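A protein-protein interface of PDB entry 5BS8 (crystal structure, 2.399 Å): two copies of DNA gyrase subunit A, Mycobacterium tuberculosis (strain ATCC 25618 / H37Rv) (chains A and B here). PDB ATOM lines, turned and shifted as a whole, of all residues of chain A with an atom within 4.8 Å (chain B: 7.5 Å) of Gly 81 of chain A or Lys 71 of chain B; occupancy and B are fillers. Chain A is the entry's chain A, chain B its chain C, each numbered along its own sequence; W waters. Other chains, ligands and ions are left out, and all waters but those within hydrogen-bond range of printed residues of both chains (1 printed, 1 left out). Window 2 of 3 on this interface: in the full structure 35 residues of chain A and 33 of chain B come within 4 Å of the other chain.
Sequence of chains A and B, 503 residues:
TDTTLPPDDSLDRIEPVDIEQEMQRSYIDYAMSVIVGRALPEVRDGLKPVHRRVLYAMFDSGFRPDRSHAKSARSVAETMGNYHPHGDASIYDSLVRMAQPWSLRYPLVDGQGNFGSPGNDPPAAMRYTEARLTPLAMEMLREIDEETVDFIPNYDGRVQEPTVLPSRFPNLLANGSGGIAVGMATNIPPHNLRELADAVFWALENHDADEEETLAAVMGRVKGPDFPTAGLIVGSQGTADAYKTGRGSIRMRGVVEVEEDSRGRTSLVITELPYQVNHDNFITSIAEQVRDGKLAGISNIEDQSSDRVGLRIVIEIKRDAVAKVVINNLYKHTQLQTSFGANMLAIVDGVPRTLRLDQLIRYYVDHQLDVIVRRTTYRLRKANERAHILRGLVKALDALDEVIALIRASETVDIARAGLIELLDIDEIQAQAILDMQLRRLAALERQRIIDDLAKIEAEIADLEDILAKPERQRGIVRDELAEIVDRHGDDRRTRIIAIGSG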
ATOM      1  N   VAL A  76     -18.239 -15.398   7.963  1.00  0.00           N
ATOM      2  CA  VAL A  76     -17.396 -15.730   6.826  1.00  0.00           C
ATOM      3  C   VAL A  76     -18.156 -15.527   5.521  1.00  0.00           C
ATOM      4  O   VAL A  76     -17.680 -14.833   4.620  1.00  0.00           O
ATOM      5  CB  VAL A  76     -16.894 -17.178   6.912  1.00  0.00           C
ATOM      6  CG1 VAL A  76     -16.103 -17.546   5.669  1.00  0.00           C
ATOM      7  CG2 VAL A  76     -16.036 -17.354   8.149  1.00  0.00           C
ATOM      8  N   ALA A  77     -19.340 -16.122   5.429  1.00  0.00           N
ATOM      9  CA  ALA A  77     -20.132 -16.068   4.204  1.00  0.00           C
ATOM     10  C   ALA A  77     -20.482 -14.633   3.822  1.00  0.00           C
ATOM     11  O   ALA A  77     -20.434 -14.269   2.649  1.00  0.00           O
ATOM     12  CB  ALA A  77     -21.398 -16.892   4.361  1.00  0.00           C
ATOM     13  N   GLU A  78     -20.838 -13.819   4.809  1.00  0.00           N
ATOM     14  CA  GLU A  78     -21.203 -12.432   4.543  1.00  0.00           C
ATOM     15  C   GLU A  78     -20.001 -11.633   4.049  1.00  0.00           C
ATOM     16  O   GLU A  78     -20.124 -10.812   3.142  1.00  0.00           O
ATOM     17  CB  GLU A  78     -21.796 -11.783   5.793  1.00  0.00           C
ATOM     18  CG  GLU A  78     -23.314 -11.835   5.839  1.00  0.00           C
ATOM     19  CD  GLU A  78     -23.961 -10.913   4.821  1.00  0.00           C
ATOM     20  OE1 GLU A  78     -23.440  -9.795   4.611  1.00  0.00           O
ATOM     21  OE2 GLU A  78     -24.986 -11.306   4.226  1.00  0.00           O
ATOM     22  N   THR A  79     -18.842 -11.881   4.648  1.00  0.00           N
ATOM     23  CA  THR A  79     -17.611 -11.221   4.233  1.00  0.00           C
ATOM     24  C   THR A  79     -17.246 -11.647   2.818  1.00  0.00           C
ATOM     25  O   THR A  79     -16.915 -10.825   1.963  1.00  0.00           O
ATOM     26  CB  THR A  79     -16.447 -11.555   5.183  1.00  0.00           C
ATOM     27  OG1 THR A  79     -16.844 -11.305   6.537  1.00  0.00           O
ATOM     28  CG2 THR A  79     -15.219 -10.721   4.850  1.00  0.00           C
ATOM     29  N   MET A  80     -17.325 -12.951   2.586  1.00  0.00           N
ATOM     30  CA  MET A  80     -16.945 -13.550   1.319  1.00  0.00           C
ATOM     31  C   MET A  80     -17.858 -13.108   0.188  1.00  0.00           C
ATOM     32  O   MET A  80     -17.410 -12.869  -0.935  1.00  0.00           O
ATOM     33  CB  MET A  80     -16.987 -15.067   1.450  1.00  0.00           C
ATOM     34  CG  MET A  80     -16.147 -15.819   0.449  1.00  0.00           C
ATOM     35  SD  MET A  80     -16.603 -17.567   0.352  1.00  0.00           S
ATOM     36  CE  MET A  80     -17.199 -17.881   2.017  1.00  0.00           C
ATOM     37  N   GLY A  81     -19.146 -13.001   0.496  1.00  0.00           N
ATOM     38  CA  GLY A  81     -20.158 -12.736  -0.508  1.00  0.00           C
ATOM     39  C   GLY A  81     -20.304 -11.280  -0.908  1.00  0.00           C
ATOM     40  O   GLY A  81     -20.766 -10.989  -2.011  1.00  0.00           O
ATOM     41  N   ASN A  82     -19.914 -10.367  -0.022  1.00  0.00           N
ATOM     42  CA  ASN A  82     -20.151  -8.944  -0.248  1.00  0.00           C
ATOM     43  C   ASN A  82     -18.890  -8.102  -0.398  1.00  0.00           C
ATOM     44  O   ASN A  82     -18.913  -7.086  -1.092  1.00  0.00           O
ATOM     45  CB  ASN A  82     -20.992  -8.366   0.894  1.00  0.00           C
ATOM     46  CG  ASN A  82     -22.456  -8.755   0.793  1.00  0.00           C
ATOM     47  OD1 ASN A  82     -22.908  -9.697   1.446  1.00  0.00           O
ATOM     48  ND2 ASN A  82     -23.206  -8.029  -0.030  1.00  0.00           N
ATOM     49  N   TYR A  83     -17.795  -8.515   0.242  1.00  0.00           N
ATOM     50  CA  TYR A  83     -16.619  -7.649   0.340  1.00  0.00           C
ATOM     51  C   TYR A  83     -15.302  -8.315  -0.048  1.00  0.00           C
ATOM     52  O   TYR A  83     -14.495  -7.716  -0.758  1.00  0.00           O
ATOM     53  CB  TYR A  83     -16.504  -7.102   1.765  1.00  0.00           C
ATOM     54  CG  TYR A  83     -17.804  -6.540   2.296  1.00  0.00           C
ATOM     55  CD1 TYR A  83     -18.311  -5.337   1.821  1.00  0.00           C
ATOM     56  CD2 TYR A  83     -18.524  -7.216   3.269  1.00  0.00           C
ATOM     57  CE1 TYR A  83     -19.501  -4.825   2.305  1.00  0.00           C
ATOM     58  CE2 TYR A  83     -19.713  -6.711   3.757  1.00  0.00           C
ATOM     59  CZ  TYR A  83     -20.197  -5.518   3.273  1.00  0.00           C
ATOM     60  OH  TYR A  83     -21.380  -5.017   3.763  1.00  0.00           O
ATOM     61  N   TYR A 155     -16.289  -5.307  -4.725  1.00  0.00           N
ATOM     62  CA  TYR A 155     -15.550  -5.911  -5.828  1.00  0.00           C
ATOM     63  C   TYR A 155     -16.412  -6.117  -7.078  1.00  0.00           C
ATOM     64  O   TYR A 155     -15.879  -6.386  -8.155  1.00  0.00           O
ATOM     65  CB  TYR A 155     -14.933  -7.242  -5.384  1.00  0.00           C
ATOM     66  CG  TYR A 155     -15.939  -8.312  -5.035  1.00  0.00           C
ATOM     67  CD1 TYR A 155     -16.422  -9.183  -6.003  1.00  0.00           C
ATOM     68  CD2 TYR A 155     -16.402  -8.456  -3.737  1.00  0.00           C
ATOM     69  CE1 TYR A 155     -17.340 -10.163  -5.687  1.00  0.00           C
ATOM     70  CE2 TYR A 155     -17.321  -9.434  -3.410  1.00  0.00           C
ATOM     71  CZ  TYR A 155     -17.786 -10.285  -4.391  1.00  0.00           C
ATOM     72  OH  TYR A 155     -18.701 -11.261  -4.076  1.00  0.00           O
ATOM     73  N   ARG A 158     -21.992  -4.063  -6.337  1.00  0.00           N
ATOM     74  CA  ARG A 158     -23.325  -4.316  -5.793  1.00  0.00           C
ATOM     75  C   ARG A 158     -23.607  -3.473  -4.550  1.00  0.00           C
ATOM     76  O   ARG A 158     -24.707  -2.945  -4.390  1.00  0.00           O
ATOM     77  CB  ARG A 158     -23.492  -5.800  -5.451  1.00  0.00           C
ATOM     78  CG  ARG A 158     -23.827  -6.695  -6.643  1.00  0.00           C
ATOM     79  CD  ARG A 158     -23.928  -8.170  -6.245  1.00  0.00           C
ATOM     80  NE  ARG A 158     -24.744  -8.369  -5.045  1.00  0.00           N
ATOM     81  CZ  ARG A 158     -24.271  -8.441  -3.801  1.00  0.00           C
ATOM     82  NH1 ARG A 158     -22.970  -8.334  -3.557  1.00  0.00           N
ATOM     83  NH2 ARG A 158     -25.109  -8.623  -2.788  1.00  0.00           N
ATOM     84  N   PHE B  63     -32.971 -15.230  -1.989  1.00  0.00           N
ATOM     85  CA  PHE B  63     -32.199 -15.775  -3.100  1.00  0.00           C
ATOM     86  C   PHE B  63     -33.128 -16.422  -4.128  1.00  0.00           C
ATOM     87  O   PHE B  63     -33.173 -17.644  -4.269  1.00  0.00           O
ATOM     88  CB  PHE B  63     -31.173 -16.790  -2.594  1.00  0.00           C
ATOM     89  CG  PHE B  63     -30.225 -16.238  -1.562  1.00  0.00           C
ATOM     90  CD1 PHE B  63     -30.042 -14.868  -1.412  1.00  0.00           C
ATOM     91  CD2 PHE B  63     -29.509 -17.096  -0.744  1.00  0.00           C
ATOM     92  CE1 PHE B  63     -29.166 -14.372  -0.462  1.00  0.00           C
ATOM     93  CE2 PHE B  63     -28.635 -16.604   0.205  1.00  0.00           C
ATOM     94  CZ  PHE B  63     -28.462 -15.243   0.347  1.00  0.00           C
ATOM     95  N   SER B  68     -30.174 -11.599  -8.749  1.00  0.00           N
ATOM     96  CA  SER B  68     -28.960 -12.275  -9.190  1.00  0.00           C
ATOM     97  C   SER B  68     -28.544 -13.369  -8.216  1.00  0.00           C
ATOM     98  O   SER B  68     -28.852 -13.306  -7.025  1.00  0.00           O
ATOM     99  CB  SER B  68     -27.822 -11.270  -9.358  1.00  0.00           C
ATOM    100  OG  SER B  68     -27.528 -10.630  -8.131  1.00  0.00           O
ATOM    101  N   HIS B  69     -27.840 -14.368  -8.739  1.00  0.00           N
ATOM    102  CA  HIS B  69     -27.365 -15.481  -7.930  1.00  0.00           C
ATOM    103  C   HIS B  69     -26.558 -14.973  -6.746  1.00  0.00           C
ATOM    104  O   HIS B  69     -25.664 -14.144  -6.903  1.00  0.00           O
ATOM    105  CB  HIS B  69     -26.511 -16.438  -8.765  1.00  0.00           C
ATOM    106  CG  HIS B  69     -27.267 -17.139  -9.849  1.00  0.00           C
ATOM    107  ND1 HIS B  69     -27.696 -16.498 -10.993  1.00  0.00           N
ATOM    108  CD2 HIS B  69     -27.665 -18.427  -9.968  1.00  0.00           C
ATOM    109  CE1 HIS B  69     -28.330 -17.365 -11.766  1.00  0.00           C
ATOM    110  NE2 HIS B  69     -28.324 -18.540 -11.165  1.00  0.00           N
ATOM    111  N   ALA B  70     -26.897 -15.459  -5.558  1.00  0.00           N
ATOM    112  CA  ALA B  70     -26.120 -15.167  -4.363  1.00  0.00           C
ATOM    113  C   ALA B  70     -24.996 -16.186  -4.250  1.00  0.00           C
ATOM    114  O   ALA B  70     -25.130 -17.303  -4.744  1.00  0.00           O
ATOM    115  CB  ALA B  70     -27.004 -15.198  -3.131  1.00  0.00           C
ATOM    116  N   LYS B  71     -23.885 -15.800  -3.628  1.00  0.00           N
ATOM    117  CA  LYS B  71     -22.803 -16.744  -3.364  1.00  0.00           C
ATOM    118  C   LYS B  71     -23.352 -17.920  -2.567  1.00  0.00           C
ATOM    119  O   LYS B  71     -24.021 -17.732  -1.549  1.00  0.00           O
ATOM    120  CB  LYS B  71     -21.654 -16.069  -2.612  1.00  0.00           C
ATOM    121  CG  LYS B  71     -20.782 -15.177  -3.484  1.00  0.00           C
ATOM    122  CD  LYS B  71     -19.897 -15.989  -4.425  1.00  0.00           C
ATOM    123  CE  LYS B  71     -19.081 -15.091  -5.347  1.00  0.00           C
ATOM    124  NZ  LYS B  71     -18.275 -15.871  -6.334  1.00  0.00           N
ATOM    125  N   SER B  72     -23.079 -19.131  -3.040  1.00  0.00           N
ATOM    126  CA  SER B  72     -23.686 -20.327  -2.464  1.00  0.00           C
ATOM    127  C   SER B  72     -23.275 -20.520  -1.008  1.00  0.00           C
ATOM    128  O   SER B  72     -23.961 -21.206  -0.251  1.00  0.00           O
ATOM    129  CB  SER B  72     -23.316 -21.560  -3.290  1.00  0.00           C
ATOM    130  OG  SER B  72     -21.913 -21.729  -3.361  1.00  0.00           O
ATOM    131  N   ALA B  73     -22.163 -19.905  -0.617  1.00  0.00           N
ATOM    132  CA  ALA B  73     -21.701 -19.964   0.766  1.00  0.00           C
ATOM    133  C   ALA B  73     -22.716 -19.317   1.701  1.00  0.00           C
ATOM    134  O   ALA B  73     -22.862 -19.728   2.852  1.00  0.00           O
ATOM    135  CB  ALA B  73     -20.349 -19.282   0.906  1.00  0.00           C
ATOM    136  N   ARG B  74     -23.415 -18.304   1.202  1.00  0.00           N
ATOM    137  CA  ARG B  74     -24.414 -17.608   2.000  1.00  0.00           C
ATOM    138  C   ARG B  74     -25.631 -18.492   2.243  1.00  0.00           C
ATOM    139  O   ARG B  74     -26.247 -18.427   3.307  1.00  0.00           O
ATOM    140  CB  ARG B  74     -24.835 -16.306   1.320  1.00  0.00           C
ATOM    141  CG  ARG B  74     -23.707 -15.303   1.180  1.00  0.00           C
ATOM    142  CD  ARG B  74     -24.176 -14.036   0.498  1.00  0.00           C
ATOM    143  NE  ARG B  74     -25.220 -13.359   1.262  1.00  0.00           N
ATOM    144  CZ  ARG B  74     -25.881 -12.288   0.840  1.00  0.00           C
ATOM    145  NH1 ARG B  74     -25.615 -11.762  -0.350  1.00  0.00           N
ATOM    146  NH2 ARG B  74     -26.816 -11.743   1.607  1.00  0.00           N
ATOM    147  N   SER B  75     -25.978 -19.314   1.257  1.00  0.00           N
ATOM    148  CA  SER B  75     -27.092 -20.245   1.398  1.00  0.00           C
ATOM    149  C   SER B  75     -26.746 -21.333   2.403  1.00  0.00           C
ATOM    150  O   SER B  75     -27.555 -21.670   3.266  1.00  0.00           O
ATOM    151  CB  SER B  75     -27.461 -20.872   0.052  1.00  0.00           C
ATOM    152  OG  SER B  75     -28.064 -19.921  -0.806  1.00  0.00           O
ATOM    153  N   VAL B  76     -25.539 -21.878   2.286  1.00  0.00           N
ATOM    154  CA  VAL B  76     -25.068 -22.887   3.222  1.00  0.00           C
ATOM    155  C   VAL B  76     -25.025 -22.325   4.635  1.00  0.00           C
ATOM    156  O   VAL B  76     -25.505 -22.958   5.573  1.00  0.00           O
ATOM    157  CB  VAL B  76     -23.672 -23.403   2.837  1.00  0.00           C
ATOM    158  CG1 VAL B  76     -23.130 -24.344   3.901  1.00  0.00           C
ATOM    159  CG2 VAL B  76     -23.728 -24.112   1.502  1.00  0.00           C
ATOM    160  N   ALA B  77     -24.446 -21.138   4.781  1.00  0.00           N
ATOM    161  CA  ALA B  77     -24.288 -20.518   6.093  1.00  0.00           C
ATOM    162  C   ALA B  77     -25.641 -20.229   6.737  1.00  0.00           C
ATOM    163  O   ALA B  77     -25.817 -20.421   7.939  1.00  0.00           O
ATOM    164  CB  ALA B  77     -23.473 -19.236   5.979  1.00  0.00           C
ATOM    165  N   LEU B  95     -27.049 -29.083  -1.633  1.00  0.00           N
ATOM    166  CA  LEU B  95     -27.450 -27.931  -2.432  1.00  0.00           C
ATOM    167  C   LEU B  95     -27.016 -28.119  -3.877  1.00  0.00           C
ATOM    168  O   LEU B  95     -27.769 -27.827  -4.804  1.00  0.00           O
ATOM    169  CB  LEU B  95     -26.855 -26.639  -1.863  1.00  0.00           C
ATOM    170  CG  LEU B  95     -27.106 -25.353  -2.660  1.00  0.00           C
ATOM    171  CD1 LEU B  95     -27.286 -24.169  -1.718  1.00  0.00           C
ATOM    172  CD2 LEU B  95     -25.972 -25.066  -3.639  1.00  0.00           C
ATOM    173  N   GLN B 112     -24.896 -21.410 -10.647  1.00  0.00           N
ATOM    174  CA  GLN B 112     -24.013 -20.650 -11.521  1.00  0.00           C
ATOM    175  C   GLN B 112     -22.563 -20.988 -11.206  1.00  0.00           C
ATOM    176  O   GLN B 112     -22.091 -20.777 -10.089  1.00  0.00           O
ATOM    177  CB  GLN B 112     -24.268 -19.149 -11.370  1.00  0.00           C
ATOM    178  CG  GLN B 112     -23.299 -18.276 -12.147  1.00  0.00           C
ATOM    179  CD  GLN B 112     -23.830 -16.873 -12.365  1.00  0.00           C
ATOM    180  OE1 GLN B 112     -23.316 -15.907 -11.801  1.00  0.00           O
ATOM    181  NE2 GLN B 112     -24.863 -16.754 -13.195  1.00  0.00           N
ATOM    182  N   MET B 126     -17.293 -24.455  -2.712  1.00  0.00           N
ATOM    183  CA  MET B 126     -18.313 -23.494  -2.313  1.00  0.00           C
ATOM    184  C   MET B 126     -17.969 -22.053  -2.700  1.00  0.00           C
ATOM    185  O   MET B 126     -18.841 -21.289  -3.112  1.00  0.00           O
ATOM    186  CB  MET B 126     -18.506 -23.593  -0.800  1.00  0.00           C
ATOM    187  CG  MET B 126     -19.703 -22.865  -0.244  1.00  0.00           C
ATOM    188  SD  MET B 126     -19.895 -23.227   1.514  1.00  0.00           S
ATOM    189  CE  MET B 126     -18.381 -22.540   2.194  1.00  0.00           C
ATOM    190  N   ARG B 127     -16.695 -21.695  -2.583  1.00  0.00           N
ATOM    191  CA  ARG B 127     -16.252 -20.326  -2.825  1.00  0.00           C
ATOM    192  C   ARG B 127     -16.450 -19.899  -4.274  1.00  0.00           C
ATOM    193  O   ARG B 127     -16.636 -18.719  -4.560  1.00  0.00           O
ATOM    194  CB  ARG B 127     -14.779 -20.176  -2.444  1.00  0.00           C
ATOM    195  CG  ARG B 127     -13.838 -20.990  -3.320  1.00  0.00           C
ATOM    196  CD  ARG B 127     -12.416 -20.999  -2.783  1.00  0.00           C
ATOM    197  NE  ARG B 127     -12.323 -21.638  -1.473  1.00  0.00           N
ATOM    198  CZ  ARG B 127     -11.181 -21.870  -0.832  1.00  0.00           C
ATOM    199  NH1 ARG B 127     -10.022 -21.520  -1.377  1.00  0.00           N
ATOM    200  NH2 ARG B 127     -11.199 -22.454   0.357  1.00  0.00           N
ATOM    201  N   PTR B 128     -16.505 -20.840  -5.187  1.00  0.00           N
ATOM    202  CA  PTR B 128     -16.480 -20.519  -6.602  1.00  0.00           C
ATOM    203  C   PTR B 128     -17.816 -20.498  -7.199  1.00  0.00           C
ATOM    204  O   PTR B 128     -17.979 -20.057  -8.347  1.00  0.00           O
ATOM    205  CB  PTR B 128     -15.731 -21.570  -7.330  1.00  0.00           C
ATOM    206  CG  PTR B 128     -14.281 -21.702  -7.006  1.00  0.00           C
ATOM    207  CD1 PTR B 128     -13.830 -22.872  -6.472  1.00  0.00           C
ATOM    208  CD2 PTR B 128     -13.378 -20.712  -7.277  1.00  0.00           C
ATOM    209  CE1 PTR B 128     -12.505 -23.037  -6.177  1.00  0.00           C
ATOM    210  CE2 PTR B 128     -12.039 -20.892  -6.976  1.00  0.00           C
ATOM    211  CZ  PTR B 128     -11.599 -22.052  -6.432  1.00  0.00           C
ATOM    212  OH  PTR B 128     -10.285 -22.200  -6.138  1.00  0.00           O
ATOM    213  P   PTR B 128      -9.625 -23.579  -6.360  1.00  0.00           P
ATOM    214  O1P PTR B 128     -10.066 -24.211  -7.646  1.00  0.00           O
ATOM    215  O2P PTR B 128      -9.886 -24.476  -5.226  1.00  0.00           O
ATOM    216  O3P PTR B 128      -8.144 -23.406  -6.464  1.00  0.00           O
ATOM    217  N   THR B 129     -18.814 -20.987  -6.502  1.00  0.00           N
ATOM    218  CA  THR B 129     -20.136 -21.135  -7.100  1.00  0.00           C
ATOM    219  C   THR B 129     -21.156 -20.171  -6.506  1.00  0.00           C
ATOM    220  O   THR B 129     -21.054 -19.777  -5.345  1.00  0.00           O
ATOM    221  CB  THR B 129     -20.659 -22.572  -6.933  1.00  0.00           C
ATOM    222  OG1 THR B 129     -20.887 -22.842  -5.544  1.00  0.00           O
ATOM    223  CG2 THR B 129     -19.658 -23.575  -7.496  1.00  0.00           C
ATOM    224  N   GLU B 130     -22.132 -19.790  -7.326  1.00  0.00           N
ATOM    225  CA  GLU B 130     -23.274 -19.002  -6.880  1.00  0.00           C
ATOM    226  C   GLU B 130     -24.545 -19.825  -7.079  1.00  0.00           C
ATOM    227  O   GLU B 130     -24.547 -20.787  -7.844  1.00  0.00           O
ATOM    228  CB  GLU B 130     -23.355 -17.678  -7.643  1.00  0.00           C
ATOM    229  CG  GLU B 130     -22.150 -16.770  -7.443  1.00  0.00           C
ATOM    230  CD  GLU B 130     -22.276 -15.456  -8.189  1.00  0.00           C
ATOM    231  OE1 GLU B 130     -23.172 -15.345  -9.051  1.00  0.00           O
ATOM    232  OE2 GLU B 130     -21.481 -14.531  -7.912  1.00  0.00           O
ATOM    233  N   ALA B 131     -25.624 -19.460  -6.393  1.00  0.00           N
ATOM    234  CA  ALA B 131     -26.843 -20.256  -6.454  1.00  0.00           C
ATOM    235  C   ALA B 131     -28.087 -19.466  -6.063  1.00  0.00           C
ATOM    236  O   ALA B 131     -28.029 -18.543  -5.250  1.00  0.00           O
ATOM    237  CB  ALA B 131     -26.704 -21.482  -5.559  1.00  0.00           C
ATOM    238  N   ARG B 132     -29.214 -19.839  -6.655  1.00  0.00           N
ATOM    239  CA  ARG B 132     -30.499 -19.271  -6.289  1.00  0.00           C
ATOM    240  C   ARG B 132     -31.568 -20.301  -6.595  1.00  0.00           C
ATOM    241  O   ARG B 132     -31.296 -21.312  -7.240  1.00  0.00           O
ATOM    242  CB  ARG B 132     -30.767 -17.967  -7.042  1.00  0.00           C
ATOM    243  CG  ARG B 132     -30.951 -18.146  -8.538  1.00  0.00           C
ATOM    244  CD  ARG B 132     -31.061 -16.810  -9.251  1.00  0.00           C
ATOM    245  NE  ARG B 132     -31.264 -16.978 -10.687  1.00  0.00           N
ATOM    246  CZ  ARG B 132     -31.267 -15.981 -11.567  1.00  0.00           C
ATOM    247  NH1 ARG B 132     -31.073 -14.733 -11.164  1.00  0.00           N
ATOM    248  NH2 ARG B 132     -31.458 -16.233 -12.854  1.00  0.00           N
HETATM  249  O   HOH W   1     -26.464 -13.825   3.630  1.00  0.00           O
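Printed residues of chain B within 4 Å of Met 80 of chain A: Ala 73 (3.6 Å).
Gly 81 of chain A touches one residue of chain B.
Printed residues of chain B within 4 Å of Asn 82 of chain A: Arg 74 (3.8 Å).
His 69 of chain B touches none of the printed residues of chain A.
Lys 71 of chain B touches just one residue of chain A: Gly 81 (3.9 Å).
Printed residues of chain A within 4 Å of Ala 73 of chain B: Ala 77 and Met 80.
Of the printed residues of chain A, Arg 74 of chain B touches Ala 77 (3.7 Å), Glu 78 (3.2 Å) and Asn 82 (3.8 Å).
Printed residues of chain A within 4 Å of Ala 77 of chain B: Ala 77.
The nearest residue of chain B that does not touch Gly 81 of chain A is Arg 74 of chain B (4.3 Å).
Water W1 bridges NE of Arg 74 of chain B (2.7 Å) and OE2 of Glu 78 of chain A (3.0 Å).
OE2 of Glu 78 of chain A is in salt-bridge range of NH2 of Arg 74 of chain B (3.2 Å).
The side-chain amide oxygen (OD1) of Asn 82 of chain A lies close to the side-chain carboxylate (OE1) of Glu 78 of chain A (3.2 Å).
The backbone carbonyl oxygen (O) of Gly 81 of chain A is in hydrogen-bond range of the side-chain hydroxyl (OH) of Tyr 155 of chain A.
ND2 of Asn 82 of chain A lies close to NH2 of Arg 158 of chain A, 3.4 Å away.
The side-chain carboxylate (OE2) of Glu 130 of chain B lies within salt-bridge range of the side-chain amino group (NZ) of Lys 71 of chain B (3.8 Å).
Ala 77 of chain B touches its own counterpart, Ala 77 of chain A.
2 positions are printed for both chains.
Of the 20 printed residues of chain B, 4 touch a printed residue of chain A.
Printed residues of chain B that touch a printed residue of chain A: Lys 71, Ala 73, Arg 74 and Ala 77.
Hydrophobic or aromatic side chains of chain B within 4 Å of the printed part of chain A: Ala 73 and Ala 77.
Hydrophobic or aromatic side chains of chain A within 4 Å of the printed part of chain B: Ala 77 and Met 80.
Among the printed residues, 7 pairs touch across the chains.
Among the printed residues, Asp or Glu carboxylates within 4 Å of a Lys or Arg side-chain nitrogen of the other chain: Glu 78 of chain A with Arg 74 of chain B.
Among the printed residues, pairs that only touch across the chains: Ala 77 of chain A with Ala 73 of chain B (3.5 Å), Ala 77 of chain A with Arg 74 of chain B (3.7 Å), Ala 77 of chain A with Ala 77 of chain B (3.5 Å), Met 80 of chain A with Ala 73 of chain B (3.6 Å), Gly 81 of chain A with Lys 71 of chain B (3.9 Å) and Asn 82 of chain A with Arg 74 of chain B (3.8 Å).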
